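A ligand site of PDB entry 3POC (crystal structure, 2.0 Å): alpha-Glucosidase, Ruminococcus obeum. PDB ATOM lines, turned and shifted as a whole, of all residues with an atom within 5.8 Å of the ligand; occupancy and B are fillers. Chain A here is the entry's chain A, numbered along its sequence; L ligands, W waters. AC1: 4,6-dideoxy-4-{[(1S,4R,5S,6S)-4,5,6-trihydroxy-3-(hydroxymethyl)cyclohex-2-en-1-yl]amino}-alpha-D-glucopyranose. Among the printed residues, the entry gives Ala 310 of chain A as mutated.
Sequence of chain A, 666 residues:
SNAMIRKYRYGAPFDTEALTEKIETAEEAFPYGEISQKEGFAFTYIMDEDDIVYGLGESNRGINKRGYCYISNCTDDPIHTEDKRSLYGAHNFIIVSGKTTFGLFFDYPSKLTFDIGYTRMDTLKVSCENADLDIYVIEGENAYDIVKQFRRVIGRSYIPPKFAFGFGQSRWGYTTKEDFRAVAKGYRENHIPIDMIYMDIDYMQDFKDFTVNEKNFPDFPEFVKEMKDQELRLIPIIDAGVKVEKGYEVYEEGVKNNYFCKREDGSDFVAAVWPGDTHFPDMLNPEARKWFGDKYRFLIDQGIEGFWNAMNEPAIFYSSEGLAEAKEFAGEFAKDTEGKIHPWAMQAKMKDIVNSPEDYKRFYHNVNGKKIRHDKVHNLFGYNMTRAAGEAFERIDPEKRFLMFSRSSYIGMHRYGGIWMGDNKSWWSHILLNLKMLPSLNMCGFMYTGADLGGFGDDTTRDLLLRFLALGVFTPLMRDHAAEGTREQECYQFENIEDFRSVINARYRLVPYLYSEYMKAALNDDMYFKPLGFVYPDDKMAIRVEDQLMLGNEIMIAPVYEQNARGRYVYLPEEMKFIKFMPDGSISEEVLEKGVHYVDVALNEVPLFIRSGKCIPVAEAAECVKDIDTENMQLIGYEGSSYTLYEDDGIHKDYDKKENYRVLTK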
ATOM      1  N   ASP A  76     -11.467   5.448 -27.239  1.00  0.00           N
ATOM      2  CA  ASP A  76     -12.183   5.095 -26.029  1.00  0.00           C
ATOM      3  C   ASP A  76     -12.547   6.372 -25.299  1.00  0.00           C
ATOM      4  O   ASP A  76     -11.784   6.818 -24.440  1.00  0.00           O
ATOM      5  CB  ASP A  76     -11.281   4.228 -25.140  1.00  0.00           C
ATOM      6  CG  ASP A  76     -11.946   3.835 -23.836  1.00  0.00           C
ATOM      7  OD1 ASP A  76     -11.225   3.364 -22.934  1.00  0.00           O
ATOM      8  OD2 ASP A  76     -13.168   3.991 -23.728  1.00  0.00           O
ATOM      9  N   TYR A  88     -16.007   5.460 -31.117  1.00  0.00           N
ATOM     10  CA  TYR A  88     -15.423   4.125 -31.286  1.00  0.00           C
ATOM     11  C   TYR A  88     -15.286   3.656 -32.715  1.00  0.00           C
ATOM     12  O   TYR A  88     -14.447   2.807 -33.007  1.00  0.00           O
ATOM     13  CB  TYR A  88     -16.230   3.088 -30.511  1.00  0.00           C
ATOM     14  CG  TYR A  88     -16.536   3.556 -29.112  1.00  0.00           C
ATOM     15  CD1 TYR A  88     -15.634   3.357 -28.076  1.00  0.00           C
ATOM     16  CD2 TYR A  88     -17.734   4.194 -28.832  1.00  0.00           C
ATOM     17  CE1 TYR A  88     -15.935   3.786 -26.784  1.00  0.00           C
ATOM     18  CE2 TYR A  88     -18.026   4.619 -27.555  1.00  0.00           C
ATOM     19  CZ  TYR A  88     -17.129   4.419 -26.540  1.00  0.00           C
ATOM     20  OH  TYR A  88     -17.453   4.844 -25.267  1.00  0.00           O
ATOM     21  N   TRP A 172     -21.598  -3.856 -15.015  1.00  0.00           N
ATOM     22  CA  TRP A 172     -20.218  -3.873 -14.564  1.00  0.00           C
ATOM     23  C   TRP A 172     -20.300  -3.979 -13.043  1.00  0.00           C
ATOM     24  O   TRP A 172     -20.633  -3.016 -12.368  1.00  0.00           O
ATOM     25  CB  TRP A 172     -19.528  -2.574 -14.997  1.00  0.00           C
ATOM     26  CG  TRP A 172     -18.088  -2.460 -14.591  1.00  0.00           C
ATOM     27  CD1 TRP A 172     -17.327  -3.420 -13.967  1.00  0.00           C
ATOM     28  CD2 TRP A 172     -17.243  -1.336 -14.769  1.00  0.00           C
ATOM     29  NE1 TRP A 172     -16.060  -2.942 -13.753  1.00  0.00           N
ATOM     30  CE2 TRP A 172     -15.980  -1.665 -14.237  1.00  0.00           C
ATOM     31  CE3 TRP A 172     -17.433  -0.061 -15.338  1.00  0.00           C
ATOM     32  CZ2 TRP A 172     -14.909  -0.771 -14.254  1.00  0.00           C
ATOM     33  CZ3 TRP A 172     -16.362   0.824 -15.358  1.00  0.00           C
ATOM     34  CH2 TRP A 172     -15.125   0.466 -14.812  1.00  0.00           C
ATOM     35  N   ASP A 200     -19.660  -9.206 -17.167  1.00  0.00           N
ATOM     36  CA  ASP A 200     -18.615  -8.223 -17.339  1.00  0.00           C
ATOM     37  C   ASP A 200     -17.326  -8.720 -16.698  1.00  0.00           C
ATOM     38  O   ASP A 200     -17.277  -9.822 -16.133  1.00  0.00           O
ATOM     39  CB  ASP A 200     -19.032  -6.905 -16.703  1.00  0.00           C
ATOM     40  CG  ASP A 200     -18.539  -5.713 -17.495  1.00  0.00           C
ATOM     41  OD1 ASP A 200     -17.387  -5.775 -17.993  1.00  0.00           O
ATOM     42  OD2 ASP A 200     -19.325  -4.750 -17.633  1.00  0.00           O
ATOM     43  N   ILE A 201     -16.299  -7.882 -16.763  1.00  0.00           N
ATOM     44  CA  ILE A 201     -14.914  -8.337 -16.582  1.00  0.00           C
ATOM     45  C   ILE A 201     -14.642  -9.042 -15.247  1.00  0.00           C
ATOM     46  O   ILE A 201     -13.619  -9.718 -15.104  1.00  0.00           O
ATOM     47  CB  ILE A 201     -13.912  -7.170 -16.776  1.00  0.00           C
ATOM     48  CG1 ILE A 201     -14.222  -6.026 -15.816  1.00  0.00           C
ATOM     49  CG2 ILE A 201     -13.936  -6.676 -18.215  1.00  0.00           C
ATOM     50  CD1 ILE A 201     -13.264  -4.850 -15.907  1.00  0.00           C
ATOM     51  N   ILE A 237     -17.762 -11.228 -21.532  1.00  0.00           N
ATOM     52  CA  ILE A 237     -16.934 -10.257 -22.229  1.00  0.00           C
ATOM     53  C   ILE A 237     -15.516 -10.796 -22.426  1.00  0.00           C
ATOM     54  O   ILE A 237     -14.995 -11.563 -21.608  1.00  0.00           O
ATOM     55  CB  ILE A 237     -16.850  -8.947 -21.429  1.00  0.00           C
ATOM     56  CG1 ILE A 237     -16.215  -7.831 -22.265  1.00  0.00           C
ATOM     57  CG2 ILE A 237     -16.029  -9.159 -20.168  1.00  0.00           C
ATOM     58  CD1 ILE A 237     -16.315  -6.447 -21.592  1.00  0.00           C
ATOM     59  N   ASP A 239     -11.704  -9.012 -23.560  1.00  0.00           N
ATOM     60  CA  ASP A 239     -11.012  -7.760 -23.836  1.00  0.00           C
ATOM     61  C   ASP A 239      -9.746  -7.967 -24.691  1.00  0.00           C
ATOM     62  O   ASP A 239      -9.241  -9.076 -24.832  1.00  0.00           O
ATOM     63  CB  ASP A 239     -10.675  -7.041 -22.528  1.00  0.00           C
ATOM     64  CG  ASP A 239     -11.882  -6.376 -21.888  1.00  0.00           C
ATOM     65  OD1 ASP A 239     -12.879  -6.052 -22.592  1.00  0.00           O
ATOM     66  OD2 ASP A 239     -11.837  -6.151 -20.663  1.00  0.00           O
ATOM     67  N   TRP A 274      -7.366  -3.251 -17.635  1.00  0.00           N
ATOM     68  CA  TRP A 274      -7.912  -3.768 -16.368  1.00  0.00           C
ATOM     69  C   TRP A 274      -6.956  -4.697 -15.607  1.00  0.00           C
ATOM     70  O   TRP A 274      -6.857  -4.611 -14.388  1.00  0.00           O
ATOM     71  CB  TRP A 274      -9.279  -4.451 -16.571  1.00  0.00           C
ATOM     72  CG  TRP A 274     -10.320  -3.592 -17.277  1.00  0.00           C
ATOM     73  CD1 TRP A 274     -10.884  -3.837 -18.505  1.00  0.00           C
ATOM     74  CD2 TRP A 274     -10.901  -2.367 -16.811  1.00  0.00           C
ATOM     75  NE1 TRP A 274     -11.776  -2.843 -18.817  1.00  0.00           N
ATOM     76  CE2 TRP A 274     -11.807  -1.937 -17.801  1.00  0.00           C
ATOM     77  CE3 TRP A 274     -10.756  -1.611 -15.643  1.00  0.00           C
ATOM     78  CZ2 TRP A 274     -12.554  -0.765 -17.667  1.00  0.00           C
ATOM     79  CZ3 TRP A 274     -11.495  -0.444 -15.524  1.00  0.00           C
ATOM     80  CH2 TRP A 274     -12.382  -0.030 -16.526  1.00  0.00           C
ATOM     81  N   TRP A 308     -19.160 -10.702 -26.102  1.00  0.00           N
ATOM     82  CA  TRP A 308     -18.950  -9.308 -26.476  1.00  0.00           C
ATOM     83  C   TRP A 308     -17.505  -8.898 -26.220  1.00  0.00           C
ATOM     84  O   TRP A 308     -16.858  -9.385 -25.285  1.00  0.00           O
ATOM     85  CB  TRP A 308     -19.978  -8.362 -25.820  1.00  0.00           C
ATOM     86  CG  TRP A 308     -20.082  -8.376 -24.309  1.00  0.00           C
ATOM     87  CD1 TRP A 308     -20.296  -9.460 -23.499  1.00  0.00           C
ATOM     88  CD2 TRP A 308     -20.051  -7.221 -23.432  1.00  0.00           C
ATOM     89  NE1 TRP A 308     -20.373  -9.055 -22.168  1.00  0.00           N
ATOM     90  CE2 TRP A 308     -20.223  -7.691 -22.106  1.00  0.00           C
ATOM     91  CE3 TRP A 308     -19.869  -5.845 -23.640  1.00  0.00           C
ATOM     92  CZ2 TRP A 308     -20.222  -6.836 -20.997  1.00  0.00           C
ATOM     93  CZ3 TRP A 308     -19.858  -4.999 -22.537  1.00  0.00           C
ATOM     94  CH2 TRP A 308     -20.042  -5.493 -21.230  1.00  0.00           C
ATOM     95  N   ALA A 310     -14.816  -5.700 -25.658  1.00  0.00           N
ATOM     96  CA  ALA A 310     -14.604  -4.286 -25.333  1.00  0.00           C
ATOM     97  C   ALA A 310     -13.107  -3.889 -25.417  1.00  0.00           C
ATOM     98  O   ALA A 310     -12.240  -4.742 -25.673  1.00  0.00           O
ATOM     99  CB  ALA A 310     -15.165  -3.973 -23.966  1.00  0.00           C
ATOM    100  N   MET A 311     -12.833  -2.605 -25.218  1.00  0.00           N
ATOM    101  CA  MET A 311     -11.468  -2.091 -25.177  1.00  0.00           C
ATOM    102  C   MET A 311     -10.670  -2.371 -26.459  1.00  0.00           C
ATOM    103  O   MET A 311      -9.438  -2.372 -26.424  1.00  0.00           O
ATOM    104  CB  MET A 311     -10.722  -2.692 -23.980  1.00  0.00           C
ATOM    105  CG  MET A 311     -11.533  -2.801 -22.709  1.00  0.00           C
ATOM    106  SD  MET A 311     -12.303  -1.239 -22.198  1.00  0.00           S
ATOM    107  CE  MET A 311     -10.913  -0.438 -21.346  1.00  0.00           C
ATOM    108  N   ARG A 407     -17.130  -3.133 -29.521  1.00  0.00           N
ATOM    109  CA  ARG A 407     -17.233  -1.694 -29.291  1.00  0.00           C
ATOM    110  C   ARG A 407     -16.690  -0.950 -30.503  1.00  0.00           C
ATOM    111  O   ARG A 407     -17.437  -0.271 -31.208  1.00  0.00           O
ATOM    112  CB  ARG A 407     -16.494  -1.289 -28.021  1.00  0.00           C
ATOM    113  CG  ARG A 407     -16.848   0.107 -27.509  1.00  0.00           C
ATOM    114  CD  ARG A 407     -16.346   0.289 -26.093  1.00  0.00           C
ATOM    115  NE  ARG A 407     -14.900   0.453 -26.023  1.00  0.00           N
ATOM    116  CZ  ARG A 407     -14.241   0.709 -24.889  1.00  0.00           C
ATOM    117  NH1 ARG A 407     -12.920   0.860 -24.897  1.00  0.00           N
ATOM    118  NH2 ARG A 407     -14.925   0.815 -23.753  1.00  0.00           N
ATOM    119  N   TRP A 420     -22.300  -2.356 -30.237  1.00  0.00           N
ATOM    120  CA  TRP A 420     -23.162  -1.568 -29.365  1.00  0.00           C
ATOM    121  C   TRP A 420     -22.534  -0.192 -29.305  1.00  0.00           C
ATOM    122  O   TRP A 420     -21.359  -0.041 -29.614  1.00  0.00           O
ATOM    123  CB  TRP A 420     -23.341  -2.217 -28.004  1.00  0.00           C
ATOM    124  CG  TRP A 420     -22.391  -1.810 -26.925  1.00  0.00           C
ATOM    125  CD1 TRP A 420     -22.604  -0.871 -25.942  1.00  0.00           C
ATOM    126  CD2 TRP A 420     -21.101  -2.372 -26.658  1.00  0.00           C
ATOM    127  NE1 TRP A 420     -21.521  -0.811 -25.112  1.00  0.00           N
ATOM    128  CE2 TRP A 420     -20.584  -1.726 -25.522  1.00  0.00           C
ATOM    129  CE3 TRP A 420     -20.334  -3.376 -27.269  1.00  0.00           C
ATOM    130  CZ2 TRP A 420     -19.326  -2.028 -25.001  1.00  0.00           C
ATOM    131  CZ3 TRP A 420     -19.096  -3.680 -26.744  1.00  0.00           C
ATOM    132  CH2 TRP A 420     -18.604  -3.006 -25.624  1.00  0.00           C
ATOM    133  N   GLY A 422     -21.427   1.784 -27.218  1.00  0.00           N
ATOM    134  CA  GLY A 422     -20.397   2.110 -26.248  1.00  0.00           C
ATOM    135  C   GLY A 422     -20.918   2.718 -24.951  1.00  0.00           C
ATOM    136  O   GLY A 422     -22.052   2.463 -24.529  1.00  0.00           O
ATOM    137  N   ASP A 423     -20.067   3.506 -24.319  1.00  0.00           N
ATOM    138  CA  ASP A 423     -20.350   4.028 -22.990  1.00  0.00           C
ATOM    139  C   ASP A 423     -21.115   5.341 -23.102  1.00  0.00           C
ATOM    140  O   ASP A 423     -20.524   6.421 -23.019  1.00  0.00           O
ATOM    141  CB  ASP A 423     -19.051   4.218 -22.196  1.00  0.00           C
ATOM    142  CG  ASP A 423     -18.234   2.939 -22.059  1.00  0.00           C
ATOM    143  OD1 ASP A 423     -17.044   3.023 -21.698  1.00  0.00           O
ATOM    144  OD2 ASP A 423     -18.794   1.841 -22.324  1.00  0.00           O
ATOM    145  N   ASP A 452     -26.687   1.279 -24.620  1.00  0.00           N
ATOM    146  CA  ASP A 452     -26.947   0.852 -23.244  1.00  0.00           C
ATOM    147  C   ASP A 452     -28.217   1.514 -22.725  1.00  0.00           C
ATOM    148  O   ASP A 452     -28.228   2.716 -22.452  1.00  0.00           O
ATOM    149  CB  ASP A 452     -25.761   1.151 -22.332  1.00  0.00           C
ATOM    150  CG  ASP A 452     -24.594   0.206 -22.562  1.00  0.00           C
ATOM    151  OD1 ASP A 452     -24.687  -0.625 -23.483  1.00  0.00           O
ATOM    152  OD2 ASP A 452     -23.580   0.291 -21.816  1.00  0.00           O
ATOM    153  N   PHE A 456     -25.338   4.021 -19.800  1.00  0.00           N
ATOM    154  CA  PHE A 456     -24.240   3.334 -19.133  1.00  0.00           C
ATOM    155  C   PHE A 456     -23.730   4.143 -17.946  1.00  0.00           C
ATOM    156  O   PHE A 456     -23.814   3.707 -16.792  1.00  0.00           O
ATOM    157  CB  PHE A 456     -23.116   3.064 -20.127  1.00  0.00           C
ATOM    158  CG  PHE A 456     -21.879   2.444 -19.506  1.00  0.00           C
ATOM    159  CD1 PHE A 456     -20.704   3.193 -19.365  1.00  0.00           C
ATOM    160  CD2 PHE A 456     -21.892   1.132 -19.063  1.00  0.00           C
ATOM    161  CE1 PHE A 456     -19.564   2.637 -18.794  1.00  0.00           C
ATOM    162  CE2 PHE A 456     -20.760   0.562 -18.486  1.00  0.00           C
ATOM    163  CZ  PHE A 456     -19.586   1.315 -18.353  1.00  0.00           C
ATOM    164  N   ARG A 479     -30.481  -4.146 -24.625  1.00  0.00           N
ATOM    165  CA  ARG A 479     -29.943  -4.531 -23.332  1.00  0.00           C
ATOM    166  C   ARG A 479     -29.783  -3.361 -22.411  1.00  0.00           C
ATOM    167  O   ARG A 479     -29.429  -2.259 -22.833  1.00  0.00           O
ATOM    168  CB  ARG A 479     -28.616  -5.285 -23.470  1.00  0.00           C
ATOM    169  CG  ARG A 479     -27.443  -4.382 -23.650  1.00  0.00           C
ATOM    170  CD  ARG A 479     -26.113  -5.095 -23.358  1.00  0.00           C
ATOM    171  NE  ARG A 479     -25.027  -4.139 -23.540  1.00  0.00           N
ATOM    172  CZ  ARG A 479     -23.743  -4.407 -23.367  1.00  0.00           C
ATOM    173  NH1 ARG A 479     -23.340  -5.623 -22.997  1.00  0.00           N
ATOM    174  NH2 ARG A 479     -22.856  -3.446 -23.569  1.00  0.00           N
ATOM    175  N   HIS A 481     -27.618  -2.032 -19.574  1.00  0.00           N
ATOM    176  CA  HIS A 481     -26.277  -2.166 -19.009  1.00  0.00           C
ATOM    177  C   HIS A 481     -25.852  -0.872 -18.305  1.00  0.00           C
ATOM    178  O   HIS A 481     -26.241   0.222 -18.719  1.00  0.00           O
ATOM    179  CB  HIS A 481     -25.286  -2.549 -20.124  1.00  0.00           C
ATOM    180  CG  HIS A 481     -23.905  -2.822 -19.639  1.00  0.00           C
ATOM    181  ND1 HIS A 481     -23.625  -3.776 -18.682  1.00  0.00           N
ATOM    182  CD2 HIS A 481     -22.714  -2.275 -19.979  1.00  0.00           C
ATOM    183  CE1 HIS A 481     -22.323  -3.792 -18.435  1.00  0.00           C
ATOM    184  NE2 HIS A 481     -21.749  -2.896 -19.220  1.00  0.00           N
ATOM    185  N   ALA A 482     -25.073  -1.002 -17.232  1.00  0.00           N
ATOM    186  CA  ALA A 482     -24.753   0.135 -16.350  1.00  0.00           C
ATOM    187  C   ALA A 482     -23.311   0.071 -15.866  1.00  0.00           C
ATOM    188  O   ALA A 482     -22.788  -1.024 -15.615  1.00  0.00           O
ATOM    189  CB  ALA A 482     -25.712   0.151 -15.147  1.00  0.00           C
ATOM    190  N   ALA A 483     -22.670   1.240 -15.733  1.00  0.00           N
ATOM    191  CA  ALA A 483     -21.307   1.304 -15.219  1.00  0.00           C
ATOM    192  C   ALA A 483     -21.282   1.029 -13.707  1.00  0.00           C
ATOM    193  O   ALA A 483     -22.308   1.143 -13.048  1.00  0.00           O
ATOM    194  CB  ALA A 483     -20.682   2.674 -15.518  1.00  0.00           C
HETATM  195  C4A AC1 L   1     -17.848  -2.353 -19.769  1.00  0.00           C
HETATM  196  N4A AC1 L   1     -16.214   0.763 -20.455  1.00  0.00           N
HETATM  197  C1B AC1 L   1     -15.890  -0.528 -21.082  1.00  0.00           C
HETATM  198  C2B AC1 L   1     -17.116  -1.108 -21.807  1.00  0.00           C
HETATM  199  O2B AC1 L   1     -17.560  -0.240 -22.876  1.00  0.00           O
HETATM  200  C3B AC1 L   1     -18.252  -1.349 -20.821  1.00  0.00           C
HETATM  201  O3B AC1 L   1     -19.437  -1.814 -21.483  1.00  0.00           O
HETATM  202  O4  AC1 L   1     -18.817  -2.439 -18.731  1.00  0.00           O
HETATM  203  C5B AC1 L   1     -16.497  -2.039 -19.177  1.00  0.00           C
HETATM  204  C7B AC1 L   1     -15.551  -1.459 -19.949  1.00  0.00           C
HETATM  205  C6B AC1 L   1     -16.078  -2.755 -17.935  1.00  0.00           C
HETATM  206  O6B AC1 L   1     -15.778  -4.054 -18.470  1.00  0.00           O
HETATM  207  O   HOH W   1     -14.031  -4.052 -20.444  1.00  0.00           O
HETATM  208  O   HOH W   2     -15.994   3.889 -19.304  1.00  0.00           O
HETATM  209  O   HOH W   3     -13.628   1.963 -21.414  1.00  0.00           O
HETATM  210  O   HOH W   4     -21.059   0.247 -22.413  1.00  0.00           O
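Residues that only touch the ligand: Ile 201 (3.2 Å), Trp 420 (3.3 Å), Trp 308 (3.4 Å), Phe 456 (3.6 Å), Trp 172 (3.7 Å), Met 311 (3.8 Å), Trp 274 (3.8 Å) and Ile 237 (3.97 Å). Hydrophobic or aromatic side chains within 4 Å of the ligand: Trp 172, Ile 201, Ile 237, Trp 274, Trp 308, Met 311, Trp 420, Phe 456 and His 481.
The side-chain carboxylate (OD2) of Asp 200 sits close to a ring nitrogen (NE2) of His 481 (3.4 Å). The side-chain hydroxyl (OH) of Tyr 88 is in hydrogen-bond range of the backbone NH (N) of Asp 423. The side-chain sulfur (SD) of Met 311 lies close to the guanidinium group (NH1) of Arg 407, 3.5 Å away. OD2 of Asp 76 is in salt-bridge range of NH1 of Arg 407, at 3.4 Å. The backbone carbonyl oxygen (O) of Gly 422 sits close to the indole nitrogen (NE1) of Trp 420 (3.4 Å). The backbone carbonyl oxygen of Phe 456 sits at hydrogen-bond distance from the backbone NH of Ala 483 (2.9 Å). The backbone NH (N) of Trp 172 sits at hydrogen-bond distance from the backbone carbonyl oxygen (O) of Ala 482 (3.1 Å). The side-chain sulfur (SD) of Met 311 sits close to the indole nitrogen (NE1) of Trp 274, at 3.8 Å.
Water W1 lies within hydrogen-bond range of O6B of the ligand (2.6 Å), NE1 of Trp 274 (3.0 Å), OD2 of Asp 239 (3.0 Å) and SD of Met 311 (3.7 Å). Water W3 lies within hydrogen-bond range of NH2 of Arg 407, N4A of the ligand, OD2 of Asp 76 and SD of Met 311. Water W2 bridges the side-chain carboxylate of Asp 423 (2.8 Å) and a nitrogen (N4A) of the ligand (3.3 Å).
O6B of the ligand sits at hydrogen-bond distance from OD1 of Asp 200 (2.4 Å). The side-chain carboxylate of Asp 423 lies within salt-bridge range of a nitrogen (N4A) of the ligand, 2.7 Å away. An oxygen (O2B) of the ligand lies within hydrogen-bond range of the guanidinium group (NH2) of Arg 407. NE2 of His 481 sits at hydrogen-bond distance from O4 of the ligand (3.0 Å).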
